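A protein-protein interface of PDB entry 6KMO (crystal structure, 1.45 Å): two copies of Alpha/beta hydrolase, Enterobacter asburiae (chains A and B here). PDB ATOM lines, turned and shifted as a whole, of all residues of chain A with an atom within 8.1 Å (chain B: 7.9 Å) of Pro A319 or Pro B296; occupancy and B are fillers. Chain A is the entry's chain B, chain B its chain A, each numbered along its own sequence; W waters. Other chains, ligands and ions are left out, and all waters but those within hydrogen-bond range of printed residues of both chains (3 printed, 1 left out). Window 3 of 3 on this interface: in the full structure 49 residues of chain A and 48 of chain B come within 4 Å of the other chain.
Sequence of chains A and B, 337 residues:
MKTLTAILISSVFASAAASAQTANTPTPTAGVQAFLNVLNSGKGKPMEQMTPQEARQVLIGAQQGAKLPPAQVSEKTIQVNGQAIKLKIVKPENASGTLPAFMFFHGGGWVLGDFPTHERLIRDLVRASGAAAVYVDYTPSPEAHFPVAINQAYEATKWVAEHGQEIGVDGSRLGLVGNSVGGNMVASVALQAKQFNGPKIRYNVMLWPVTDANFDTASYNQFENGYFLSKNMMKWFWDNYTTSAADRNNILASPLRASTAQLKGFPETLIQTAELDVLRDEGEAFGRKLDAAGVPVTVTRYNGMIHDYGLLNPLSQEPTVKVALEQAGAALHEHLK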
ATOM      1  N   THR A  29     -32.228  15.244 -24.916  1.00  0.00           N
ATOM      2  CA  THR A  29     -31.616  16.562 -24.829  1.00  0.00           C
ATOM      3  C   THR A  29     -31.961  17.370 -26.084  1.00  0.00           C
ATOM      4  O   THR A  29     -32.426  16.841 -27.100  1.00  0.00           O
ATOM      5  CB  THR A  29     -30.093  16.482 -24.741  1.00  0.00           C
ATOM      6  OG1 THR A  29     -29.616  15.906 -25.964  1.00  0.00           O
ATOM      7  CG2 THR A  29     -29.607  15.715 -23.505  1.00  0.00           C
ATOM      8  N   GLY A  31     -29.957  18.738 -28.226  1.00  0.00           N
ATOM      9  CA  GLY A  31     -29.166  18.334 -29.372  1.00  0.00           C
ATOM     10  C   GLY A  31     -29.668  17.043 -29.986  1.00  0.00           C
ATOM     11  O   GLY A  31     -29.719  16.895 -31.214  1.00  0.00           O
ATOM     12  N   VAL A  32     -30.066  16.095 -29.143  1.00  0.00           N
ATOM     13  CA  VAL A  32     -30.620  14.849 -29.661  1.00  0.00           C
ATOM     14  C   VAL A  32     -31.975  15.102 -30.301  1.00  0.00           C
ATOM     15  O   VAL A  32     -32.295  14.507 -31.337  1.00  0.00           O
ATOM     16  CB  VAL A  32     -30.677  13.792 -28.546  1.00  0.00           C
ATOM     17  CG1 VAL A  32     -31.441  12.546 -29.001  1.00  0.00           C
ATOM     18  CG2 VAL A  32     -29.263  13.415 -28.114  1.00  0.00           C
ATOM     19  N   TYR A 302     -27.128   7.096 -19.271  1.00  0.00           N
ATOM     20  CA  TYR A 302     -26.908   8.478 -19.705  1.00  0.00           C
ATOM     21  C   TYR A 302     -28.252   9.061 -20.141  1.00  0.00           C
ATOM     22  O   TYR A 302     -28.869   8.597 -21.112  1.00  0.00           O
ATOM     23  CB  TYR A 302     -25.845   8.545 -20.797  1.00  0.00           C
ATOM     24  CG  TYR A 302     -24.450   8.301 -20.257  1.00  0.00           C
ATOM     25  CD1 TYR A 302     -23.982   7.023 -20.042  1.00  0.00           C
ATOM     26  CD2 TYR A 302     -23.633   9.361 -19.881  1.00  0.00           C
ATOM     27  CE1 TYR A 302     -22.736   6.790 -19.510  1.00  0.00           C
ATOM     28  CE2 TYR A 302     -22.344   9.134 -19.362  1.00  0.00           C
ATOM     29  CZ  TYR A 302     -21.926   7.845 -19.162  1.00  0.00           C
ATOM     30  OH  TYR A 302     -20.684   7.582 -18.613  1.00  0.00           O
ATOM     31  N   MET A 305     -30.341  10.566 -23.955  1.00  0.00           N
ATOM     32  CA  MET A 305     -29.671   9.966 -25.092  1.00  0.00           C
ATOM     33  C   MET A 305     -30.552   8.940 -25.782  1.00  0.00           C
ATOM     34  O   MET A 305     -31.380   8.264 -25.155  1.00  0.00           O
ATOM     35  CB  MET A 305     -28.362   9.280 -24.657  1.00  0.00           C
ATOM     36  CG  MET A 305     -27.273  10.232 -24.185  1.00  0.00           C
ATOM     37  SD  MET A 305     -26.700  11.494 -25.457  1.00  0.00           S
ATOM     38  CE  MET A 305     -27.593  12.966 -24.798  1.00  0.00           C
ATOM     39  N   LEU A 315     -23.860  13.421 -33.693  1.00  0.00           N
ATOM     40  CA  LEU A 315     -23.940  13.666 -32.263  1.00  0.00           C
ATOM     41  C   LEU A 315     -22.581  13.734 -31.575  1.00  0.00           C
ATOM     42  O   LEU A 315     -22.522  13.814 -30.339  1.00  0.00           O
ATOM     43  CB  LEU A 315     -24.795  12.598 -31.591  1.00  0.00           C
ATOM     44  CG  LEU A 315     -26.251  12.489 -32.046  1.00  0.00           C
ATOM     45  CD1 LEU A 315     -26.958  11.375 -31.316  1.00  0.00           C
ATOM     46  CD2 LEU A 315     -26.956  13.825 -31.837  1.00  0.00           C
ATOM     47  N   SER A 316     -21.489  13.759 -32.338  1.00  0.00           N
ATOM     48  CA  SER A 316     -20.165  13.671 -31.742  1.00  0.00           C
ATOM     49  C   SER A 316     -19.766  14.909 -30.948  1.00  0.00           C
ATOM     50  O   SER A 316     -18.793  14.834 -30.194  1.00  0.00           O
ATOM     51  CB  SER A 316     -19.124  13.377 -32.819  1.00  0.00           C
ATOM     52  OG  SER A 316     -18.941  14.487 -33.673  1.00  0.00           O
ATOM     53  N   GLN A 317     -20.465  16.027 -31.085  1.00  0.00           N
ATOM     54  CA  GLN A 317     -20.215  17.195 -30.256  1.00  0.00           C
ATOM     55  C   GLN A 317     -21.265  17.383 -29.166  1.00  0.00           C
ATOM     56  O   GLN A 317     -21.239  18.398 -28.450  1.00  0.00           O
ATOM     57  CB  GLN A 317     -20.096  18.458 -31.112  1.00  0.00           C
ATOM     58  CG  GLN A 317     -18.768  18.539 -31.880  1.00  0.00           C
ATOM     59  CD  GLN A 317     -17.558  18.583 -30.967  1.00  0.00           C
ATOM     60  OE1 GLN A 317     -17.520  19.351 -29.999  1.00  0.00           O
ATOM     61  NE2 GLN A 317     -16.562  17.752 -31.261  1.00  0.00           N
ATOM     62  N   GLU A 318     -22.189  16.443 -29.020  1.00  0.00           N
ATOM     63  CA  GLU A 318     -23.137  16.514 -27.923  1.00  0.00           C
ATOM     64  C   GLU A 318     -22.381  16.409 -26.601  1.00  0.00           C
ATOM     65  O   GLU A 318     -21.533  15.524 -26.448  1.00  0.00           O
ATOM     66  CB  GLU A 318     -24.142  15.379 -28.081  1.00  0.00           C
ATOM     67  CG  GLU A 318     -25.222  15.316 -27.022  1.00  0.00           C
ATOM     68  CD  GLU A 318     -26.243  16.427 -27.114  1.00  0.00           C
ATOM     69  OE1 GLU A 318     -26.329  17.103 -28.171  1.00  0.00           O
ATOM     70  OE2 GLU A 318     -26.940  16.658 -26.094  1.00  0.00           O
ATOM     71  N   PRO A 319     -22.641  17.295 -25.634  1.00  0.00           N
ATOM     72  CA  PRO A 319     -21.837  17.264 -24.403  1.00  0.00           C
ATOM     73  C   PRO A 319     -21.822  15.904 -23.733  1.00  0.00           C
ATOM     74  O   PRO A 319     -20.754  15.410 -23.337  1.00  0.00           O
ATOM     75  CB  PRO A 319     -22.486  18.351 -23.535  1.00  0.00           C
ATOM     76  CG  PRO A 319     -23.013  19.341 -24.540  1.00  0.00           C
ATOM     77  CD  PRO A 319     -23.482  18.509 -25.717  1.00  0.00           C
ATOM     78  N   THR A 320     -22.987  15.263 -23.629  1.00  0.00           N
ATOM     79  CA  THR A 320     -23.074  13.947 -22.995  1.00  0.00           C
ATOM     80  C   THR A 320     -22.234  12.912 -23.720  1.00  0.00           C
ATOM     81  O   THR A 320     -21.651  12.035 -23.085  1.00  0.00           O
ATOM     82  CB  THR A 320     -24.536  13.490 -22.971  1.00  0.00           C
ATOM     83  OG1 THR A 320     -25.264  14.367 -22.129  1.00  0.00           O
ATOM     84  CG2 THR A 320     -24.681  12.069 -22.475  1.00  0.00           C
ATOM     85  N   VAL A 321     -22.186  12.967 -25.052  1.00  0.00           N
ATOM     86  CA  VAL A 321     -21.405  12.000 -25.813  1.00  0.00           C
ATOM     87  C   VAL A 321     -19.929  12.122 -25.468  1.00  0.00           C
ATOM     88  O   VAL A 321     -19.241  11.122 -25.191  1.00  0.00           O
ATOM     89  CB  VAL A 321     -21.640  12.179 -27.322  1.00  0.00           C
ATOM     90  CG1 VAL A 321     -20.620  11.362 -28.107  1.00  0.00           C
ATOM     91  CG2 VAL A 321     -23.077  11.793 -27.688  1.00  0.00           C
ATOM     92  N   LYS A 322     -19.412  13.351 -25.473  1.00  0.00           N
ATOM     93  CA  LYS A 322     -17.988  13.540 -25.217  1.00  0.00           C
ATOM     94  C   LYS A 322     -17.629  13.059 -23.822  1.00  0.00           C
ATOM     95  O   LYS A 322     -16.608  12.387 -23.633  1.00  0.00           O
ATOM     96  CB  LYS A 322     -17.638  15.013 -25.397  1.00  0.00           C
ATOM     97  CG  LYS A 322     -17.756  15.472 -26.855  1.00  0.00           C
ATOM     98  CD  LYS A 322     -17.201  16.864 -27.099  1.00  0.00           C
ATOM     99  CE  LYS A 322     -18.101  17.932 -26.610  1.00  0.00           C
ATOM    100  NZ  LYS A 322     -17.563  19.244 -27.095  1.00  0.00           N
ATOM    101  N   VAL A 323     -18.479  13.360 -22.840  1.00  0.00           N
ATOM    102  CA  VAL A 323     -18.225  12.917 -21.474  1.00  0.00           C
ATOM    103  C   VAL A 323     -18.353  11.400 -21.359  1.00  0.00           C
ATOM    104  O   VAL A 323     -17.503  10.747 -20.748  1.00  0.00           O
ATOM    105  CB  VAL A 323     -19.126  13.668 -20.486  1.00  0.00           C
ATOM    106  CG1 VAL A 323     -19.042  13.059 -19.098  1.00  0.00           C
ATOM    107  CG2 VAL A 323     -18.707  15.123 -20.434  1.00  0.00           C
ATOM    108  N   ALA A 324     -19.403  10.816 -21.938  1.00  0.00           N
ATOM    109  CA  ALA A 324     -19.602   9.379 -21.802  1.00  0.00           C
ATOM    110  C   ALA A 324     -18.412   8.598 -22.334  1.00  0.00           C
ATOM    111  O   ALA A 324     -18.017   7.581 -21.752  1.00  0.00           O
ATOM    112  CB  ALA A 324     -20.860   8.967 -22.561  1.00  0.00           C
ATOM    113  N   LEU A 325     -17.868   9.021 -23.467  1.00  0.00           N
ATOM    114  CA  LEU A 325     -16.771   8.286 -24.089  1.00  0.00           C
ATOM    115  C   LEU A 325     -15.471   8.511 -23.330  1.00  0.00           C
ATOM    116  O   LEU A 325     -14.690   7.568 -23.146  1.00  0.00           O
ATOM    117  CB  LEU A 325     -16.669   8.645 -25.573  1.00  0.00           C
ATOM    118  CG  LEU A 325     -17.904   8.237 -26.388  1.00  0.00           C
ATOM    119  CD1 LEU A 325     -17.719   8.638 -27.853  1.00  0.00           C
ATOM    120  CD2 LEU A 325     -18.179   6.751 -26.284  1.00  0.00           C
ATOM    121  N   GLU A 326     -15.241   9.729 -22.820  1.00  0.00           N
ATOM    122  CA  GLU A 326     -14.120   9.947 -21.924  1.00  0.00           C
ATOM    123  C   GLU A 326     -14.232   9.045 -20.705  1.00  0.00           C
ATOM    124  O   GLU A 326     -13.245   8.448 -20.269  1.00  0.00           O
ATOM    125  CB  GLU A 326     -14.071  11.405 -21.501  1.00  0.00           C
ATOM    126  CG  GLU A 326     -12.886  11.757 -20.607  1.00  0.00           C
ATOM    127  CD  GLU A 326     -11.551  11.711 -21.324  1.00  0.00           C
ATOM    128  OE1 GLU A 326     -11.508  11.933 -22.557  1.00  0.00           O
ATOM    129  OE2 GLU A 326     -10.524  11.485 -20.642  1.00  0.00           O
ATOM    130  N   ARG B 202     -14.950  26.638 -14.772  1.00  0.00           N
ATOM    131  CA  ARG B 202     -14.763  25.716 -15.884  1.00  0.00           C
ATOM    132  C   ARG B 202     -15.799  24.603 -15.899  1.00  0.00           C
ATOM    133  O   ARG B 202     -16.243  24.171 -16.973  1.00  0.00           O
ATOM    134  CB  ARG B 202     -13.388  25.048 -15.792  1.00  0.00           C
ATOM    135  CG  ARG B 202     -12.235  25.914 -16.296  1.00  0.00           C
ATOM    136  CD  ARG B 202     -12.314  26.106 -17.808  1.00  0.00           C
ATOM    137  NE  ARG B 202     -11.102  26.740 -18.336  1.00  0.00           N
ATOM    138  CZ  ARG B 202     -10.011  26.074 -18.695  1.00  0.00           C
ATOM    139  NH1 ARG B 202      -9.954  24.758 -18.594  1.00  0.00           N
ATOM    140  NH2 ARG B 202      -8.958  26.732 -19.167  1.00  0.00           N
ATOM    141  N   TYR B 203     -16.164  24.078 -14.728  1.00  0.00           N
ATOM    142  CA  TYR B 203     -16.959  22.857 -14.703  1.00  0.00           C
ATOM    143  C   TYR B 203     -17.554  22.678 -13.323  1.00  0.00           C
ATOM    144  O   TYR B 203     -16.898  22.963 -12.319  1.00  0.00           O
ATOM    145  CB  TYR B 203     -16.092  21.635 -15.023  1.00  0.00           C
ATOM    146  CG  TYR B 203     -16.816  20.437 -15.592  1.00  0.00           C
ATOM    147  CD1 TYR B 203     -17.510  20.544 -16.777  1.00  0.00           C
ATOM    148  CD2 TYR B 203     -16.747  19.189 -14.976  1.00  0.00           C
ATOM    149  CE1 TYR B 203     -18.161  19.443 -17.326  1.00  0.00           C
ATOM    150  CE2 TYR B 203     -17.387  18.089 -15.516  1.00  0.00           C
ATOM    151  CZ  TYR B 203     -18.098  18.220 -16.686  1.00  0.00           C
ATOM    152  OH  TYR B 203     -18.703  17.109 -17.242  1.00  0.00           O
ATOM    153  N   ASN B 204     -18.782  22.182 -13.281  1.00  0.00           N
ATOM    154  CA  ASN B 204     -19.458  21.786 -12.055  1.00  0.00           C
ATOM    155  C   ASN B 204     -19.629  20.272 -12.051  1.00  0.00           C
ATOM    156  O   ASN B 204     -20.024  19.686 -13.065  1.00  0.00           O
ATOM    157  CB  ASN B 204     -20.872  22.357 -12.013  1.00  0.00           C
ATOM    158  CG  ASN B 204     -20.917  23.839 -11.881  1.00  0.00           C
ATOM    159  OD1 ASN B 204     -20.016  24.463 -11.324  1.00  0.00           O
ATOM    160  ND2 ASN B 204     -21.999  24.428 -12.359  1.00  0.00           N
ATOM    161  N   GLY B 265     -26.396  30.376 -19.108  1.00  0.00           N
ATOM    162  CA  GLY B 265     -25.040  30.729 -18.765  1.00  0.00           C
ATOM    163  C   GLY B 265     -24.439  29.969 -17.593  1.00  0.00           C
ATOM    164  O   GLY B 265     -23.281  30.211 -17.245  1.00  0.00           O
ATOM    165  N   PHE B 266     -25.188  29.058 -16.980  1.00  0.00           N
ATOM    166  CA  PHE B 266     -24.637  28.208 -15.924  1.00  0.00           C
ATOM    167  C   PHE B 266     -23.420  27.462 -16.476  1.00  0.00           C
ATOM    168  O   PHE B 266     -23.368  27.138 -17.661  1.00  0.00           O
ATOM    169  CB  PHE B 266     -25.734  27.196 -15.582  1.00  0.00           C
ATOM    170  CG  PHE B 266     -25.634  26.492 -14.234  1.00  0.00           C
ATOM    171  CD1 PHE B 266     -26.082  27.090 -13.065  1.00  0.00           C
ATOM    172  CD2 PHE B 266     -25.197  25.175 -14.171  1.00  0.00           C
ATOM    173  CE1 PHE B 266     -26.056  26.405 -11.865  1.00  0.00           C
ATOM    174  CE2 PHE B 266     -25.174  24.481 -12.960  1.00  0.00           C
ATOM    175  CZ  PHE B 266     -25.601  25.095 -11.817  1.00  0.00           C
ATOM    176  N   PRO B 267     -22.424  27.175 -15.639  1.00  0.00           N
ATOM    177  CA  PRO B 267     -21.240  26.465 -16.148  1.00  0.00           C
ATOM    178  C   PRO B 267     -21.572  25.069 -16.667  1.00  0.00           C
ATOM    179  O   PRO B 267     -22.558  24.444 -16.269  1.00  0.00           O
ATOM    180  CB  PRO B 267     -20.307  26.386 -14.928  1.00  0.00           C
ATOM    181  CG  PRO B 267     -20.757  27.519 -14.027  1.00  0.00           C
ATOM    182  CD  PRO B 267     -22.248  27.624 -14.247  1.00  0.00           C
ATOM    183  N   GLU B 268     -20.706  24.568 -17.539  1.00  0.00           N
ATOM    184  CA  GLU B 268     -20.798  23.180 -17.971  1.00  0.00           C
ATOM    185  C   GLU B 268     -20.824  22.284 -16.746  1.00  0.00           C
ATOM    186  O   GLU B 268     -20.087  22.510 -15.780  1.00  0.00           O
ATOM    187  CB  GLU B 268     -19.629  22.820 -18.881  1.00  0.00           C
ATOM    188  CG  GLU B 268     -19.574  23.686 -20.136  1.00  0.00           C
ATOM    189  CD  GLU B 268     -18.868  23.048 -21.315  1.00  0.00           C
ATOM    190  OE1 GLU B 268     -18.741  21.813 -21.391  1.00  0.00           O
ATOM    191  OE2 GLU B 268     -18.435  23.820 -22.202  1.00  0.00           O
ATOM    192  N   THR B 269     -21.654  21.237 -16.792  1.00  0.00           N
ATOM    193  CA  THR B 269     -22.002  20.490 -15.593  1.00  0.00           C
ATOM    194  C   THR B 269     -22.086  18.996 -15.849  1.00  0.00           C
ATOM    195  O   THR B 269     -22.560  18.553 -16.900  1.00  0.00           O
ATOM    196  CB  THR B 269     -23.353  21.001 -15.061  1.00  0.00           C
ATOM    197  OG1 THR B 269     -23.218  22.353 -14.614  1.00  0.00           O
ATOM    198  CG2 THR B 269     -23.868  20.197 -13.897  1.00  0.00           C
ATOM    199  N   LEU B 270     -21.632  18.228 -14.858  1.00  0.00           N
ATOM    200  CA  LEU B 270     -21.868  16.796 -14.747  1.00  0.00           C
ATOM    201  C   LEU B 270     -22.716  16.584 -13.502  1.00  0.00           C
ATOM    202  O   LEU B 270     -22.360  17.079 -12.424  1.00  0.00           O
ATOM    203  CB  LEU B 270     -20.558  16.029 -14.597  1.00  0.00           C
ATOM    204  CG  LEU B 270     -20.703  14.544 -14.237  1.00  0.00           C
ATOM    205  CD1 LEU B 270     -21.401  13.755 -15.334  1.00  0.00           C
ATOM    206  CD2 LEU B 270     -19.345  13.938 -13.973  1.00  0.00           C
ATOM    207  N   GLY B 287     -30.902  18.554 -14.297  1.00  0.00           N
ATOM    208  CA  GLY B 287     -30.125  18.419 -15.515  1.00  0.00           C
ATOM    209  C   GLY B 287     -30.914  18.726 -16.774  1.00  0.00           C
ATOM    210  O   GLY B 287     -30.396  19.353 -17.697  1.00  0.00           O
ATOM    211  N   LEU B 290     -31.239  22.469 -17.087  1.00  0.00           N
ATOM    212  CA  LEU B 290     -29.995  23.075 -17.548  1.00  0.00           C
ATOM    213  C   LEU B 290     -29.875  22.923 -19.055  1.00  0.00           C
ATOM    214  O   LEU B 290     -29.556  23.877 -19.768  1.00  0.00           O
ATOM    215  CB  LEU B 290     -28.804  22.435 -16.834  1.00  0.00           C
ATOM    216  CG  LEU B 290     -28.601  22.774 -15.360  1.00  0.00           C
ATOM    217  CD1 LEU B 290     -27.407  21.997 -14.844  1.00  0.00           C
ATOM    218  CD2 LEU B 290     -28.370  24.250 -15.156  1.00  0.00           C
ATOM    219  N   ASP B 291     -30.155  21.725 -19.564  1.00  0.00           N
ATOM    220  CA  ASP B 291     -30.011  21.512 -21.003  1.00  0.00           C
ATOM    221  C   ASP B 291     -30.984  22.382 -21.786  1.00  0.00           C
ATOM    222  O   ASP B 291     -30.633  22.914 -22.846  1.00  0.00           O
ATOM    223  CB  ASP B 291     -30.226  20.041 -21.326  1.00  0.00           C
ATOM    224  CG  ASP B 291     -30.076  19.740 -22.790  1.00  0.00           C
ATOM    225  OD1 ASP B 291     -28.938  19.662 -23.289  1.00  0.00           O
ATOM    226  OD2 ASP B 291     -31.130  19.565 -23.460  1.00  0.00           O
ATOM    227  N   ALA B 293     -31.852  25.263 -21.034  1.00  0.00           N
ATOM    228  CA  ALA B 293     -31.279  26.594 -20.995  1.00  0.00           C
ATOM    229  C   ALA B 293     -29.978  26.709 -21.774  1.00  0.00           C
ATOM    230  O   ALA B 293     -29.276  27.717 -21.644  1.00  0.00           O
ATOM    231  CB  ALA B 293     -31.071  27.028 -19.541  1.00  0.00           C
ATOM    232  N   GLY B 294     -29.631  25.711 -22.581  1.00  0.00           N
ATOM    233  CA  GLY B 294     -28.446  25.758 -23.404  1.00  0.00           C
ATOM    234  C   GLY B 294     -27.158  25.447 -22.689  1.00  0.00           C
ATOM    235  O   GLY B 294     -26.089  25.660 -23.260  1.00  0.00           O
ATOM    236  N   VAL B 295     -27.229  24.960 -21.456  1.00  0.00           N
ATOM    237  CA  VAL B 295     -26.037  24.625 -20.674  1.00  0.00           C
ATOM    238  C   VAL B 295     -25.527  23.262 -21.127  1.00  0.00           C
ATOM    239  O   VAL B 295     -26.313  22.309 -21.160  1.00  0.00           O
ATOM    240  CB  VAL B 295     -26.406  24.581 -19.198  1.00  0.00           C
ATOM    241  CG1 VAL B 295     -25.211  24.183 -18.343  1.00  0.00           C
ATOM    242  CG2 VAL B 295     -26.961  25.929 -18.743  1.00  0.00           C
ATOM    243  N   PRO B 296     -24.243  23.115 -21.451  1.00  0.00           N
ATOM    244  CA  PRO B 296     -23.696  21.768 -21.686  1.00  0.00           C
ATOM    245  C   PRO B 296     -23.743  20.968 -20.394  1.00  0.00           C
ATOM    246  O   PRO B 296     -23.125  21.340 -19.391  1.00  0.00           O
ATOM    247  CB  PRO B 296     -22.262  22.038 -22.158  1.00  0.00           C
ATOM    248  CG  PRO B 296     -22.299  23.486 -22.648  1.00  0.00           C
ATOM    249  CD  PRO B 296     -23.221  24.155 -21.685  1.00  0.00           C
ATOM    250  N   VAL B 297     -24.505  19.883 -20.400  1.00  0.00           N
ATOM    251  CA  VAL B 297     -24.741  19.106 -19.188  1.00  0.00           C
ATOM    252  C   VAL B 297     -24.841  17.621 -19.519  1.00  0.00           C
ATOM    253  O   VAL B 297     -25.480  17.213 -20.501  1.00  0.00           O
ATOM    254  CB  VAL B 297     -25.970  19.621 -18.411  1.00  0.00           C
ATOM    255  CG1 VAL B 297     -27.217  19.579 -19.278  1.00  0.00           C
ATOM    256  CG2 VAL B 297     -26.173  18.808 -17.157  1.00  0.00           C
ATOM    257  N   THR B 298     -24.212  16.811 -18.673  1.00  0.00           N
ATOM    258  CA  THR B 298     -24.267  15.354 -18.730  1.00  0.00           C
ATOM    259  C   THR B 298     -24.920  14.878 -17.448  1.00  0.00           C
ATOM    260  O   THR B 298     -24.545  15.336 -16.363  1.00  0.00           O
ATOM    261  CB  THR B 298     -22.850  14.781 -18.814  1.00  0.00           C
ATOM    262  OG1 THR B 298     -22.200  15.262 -19.994  1.00  0.00           O
ATOM    263  CG2 THR B 298     -22.869  13.271 -18.857  1.00  0.00           C
ATOM    264  N   VAL B 299     -25.892  13.973 -17.565  1.00  0.00           N
ATOM    265  CA  VAL B 299     -26.557  13.385 -16.403  1.00  0.00           C
ATOM    266  C   VAL B 299     -26.372  11.876 -16.467  1.00  0.00           C
ATOM    267  O   VAL B 299     -26.815  11.235 -17.428  1.00  0.00           O
ATOM    268  CB  VAL B 299     -28.047  13.732 -16.350  1.00  0.00           C
ATOM    269  CG1 VAL B 299     -28.701  13.084 -15.141  1.00  0.00           C
ATOM    270  CG2 VAL B 299     -28.248  15.257 -16.299  1.00  0.00           C
ATOM    271  N   HIS B 335     -12.015  19.242 -18.408  1.00  0.00           N
ATOM    272  CA  HIS B 335     -12.522  20.605 -18.400  1.00  0.00           C
ATOM    273  C   HIS B 335     -11.636  21.587 -17.653  1.00  0.00           C
ATOM    274  O   HIS B 335     -11.910  22.784 -17.698  1.00  0.00           O
ATOM    275  CB  HIS B 335     -13.963  20.625 -17.883  1.00  0.00           C
ATOM    276  CG  HIS B 335     -14.908  20.016 -18.853  1.00  0.00           C
ATOM    277  ND1 HIS B 335     -15.659  20.773 -19.728  1.00  0.00           N
ATOM    278  CD2 HIS B 335     -15.158  18.720 -19.158  1.00  0.00           C
ATOM    279  CE1 HIS B 335     -16.347  19.967 -20.520  1.00  0.00           C
ATOM    280  NE2 HIS B 335     -16.055  18.719 -20.199  1.00  0.00           N
HETATM  281  O   HOH W   1     -26.982  13.448 -20.197  1.00  0.00           O
HETATM  282  O   HOH W   2     -25.639  16.513 -23.749  1.00  0.00           O
HETATM  283  O   HOH W   3     -28.231  19.150 -25.925  1.00  0.00           O
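The backbone NH (N) of Val A32 lies within hydrogen-bond range of the side-chain hydroxyl (OG1) of Thr A29, at 3.2 Å. The side-chain carboxylate (OE2) of Glu A318 lies within hydrogen-bond range of the side-chain hydroxyl (OG1) of Thr A29 (2.8 Å). O of Pro B296 lies within hydrogen-bond range of N of Thr B269 (3.0 Å). N of Thr B298 sits at hydrogen-bond distance from O of Thr B269, at 3.0 Å.
Of the 20 printed residues of chain B, 6 touch a printed residue of chain A. Of the 17 printed residues of chain A, 5 touch a printed residue of chain B. Printed residues of chain A that touch a printed residue of chain B: Thr A29, Tyr A302, Pro A319, Thr A320 and Val A323. Among the printed residues, no Asp or Glu carboxylate lies within 4 Å of a Lys or Arg side-chain nitrogen of the other chain.
Water W2 lies within hydrogen-bond range of the side-chain carboxylate of Glu A318, the side-chain hydroxyl of Thr A320 and the backbone carbonyl oxygen of Val B297. Water W1 bridges OG1 of Thr A320 and N of Val B299. Water W3 lies within hydrogen-bond range of OD1 of Asp B291 (2.8 Å), OE2 of Glu A318 (2.8 Å) and N of Gly A31 (2.9 Å).
O of Val B297 lies within hydrogen-bond range of OG1 of Thr A320, at 3.3 Å.
No position is printed for both chains. Of the 8 pairs that touch across the chains among the printed residues, none has its exchanged pair printed and touching as well.
Among the printed residues, merely in contact across the chains: Thr A29 with Asp B291, Tyr A302 with Val B299, Pro A319 with Pro B296, Pro A319 with Thr B298, Thr A320 with Thr B298, Val A323 with Tyr B203 and Val A323 with Thr B298.
Printed residues of chain B within 4 Å of Thr A29: Asp B291 (3.3 Å). Printed residues of chain B within 4 Å of Tyr A302: Val B299 (3.6 Å). Arg B202 touches none of the printed residues of chain A. Of chain A, only Pro A319 comes within 4 Å of Pro B296. Printed residues of chain A within 4 Å of Thr B298: Pro A319 (3.6 Å), Thr A320 (3.4 Å) and Val A323 (3.5 Å). The nearest residue of chain A that does not touch Pro B296 is Thr A320 (6.6 Å).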
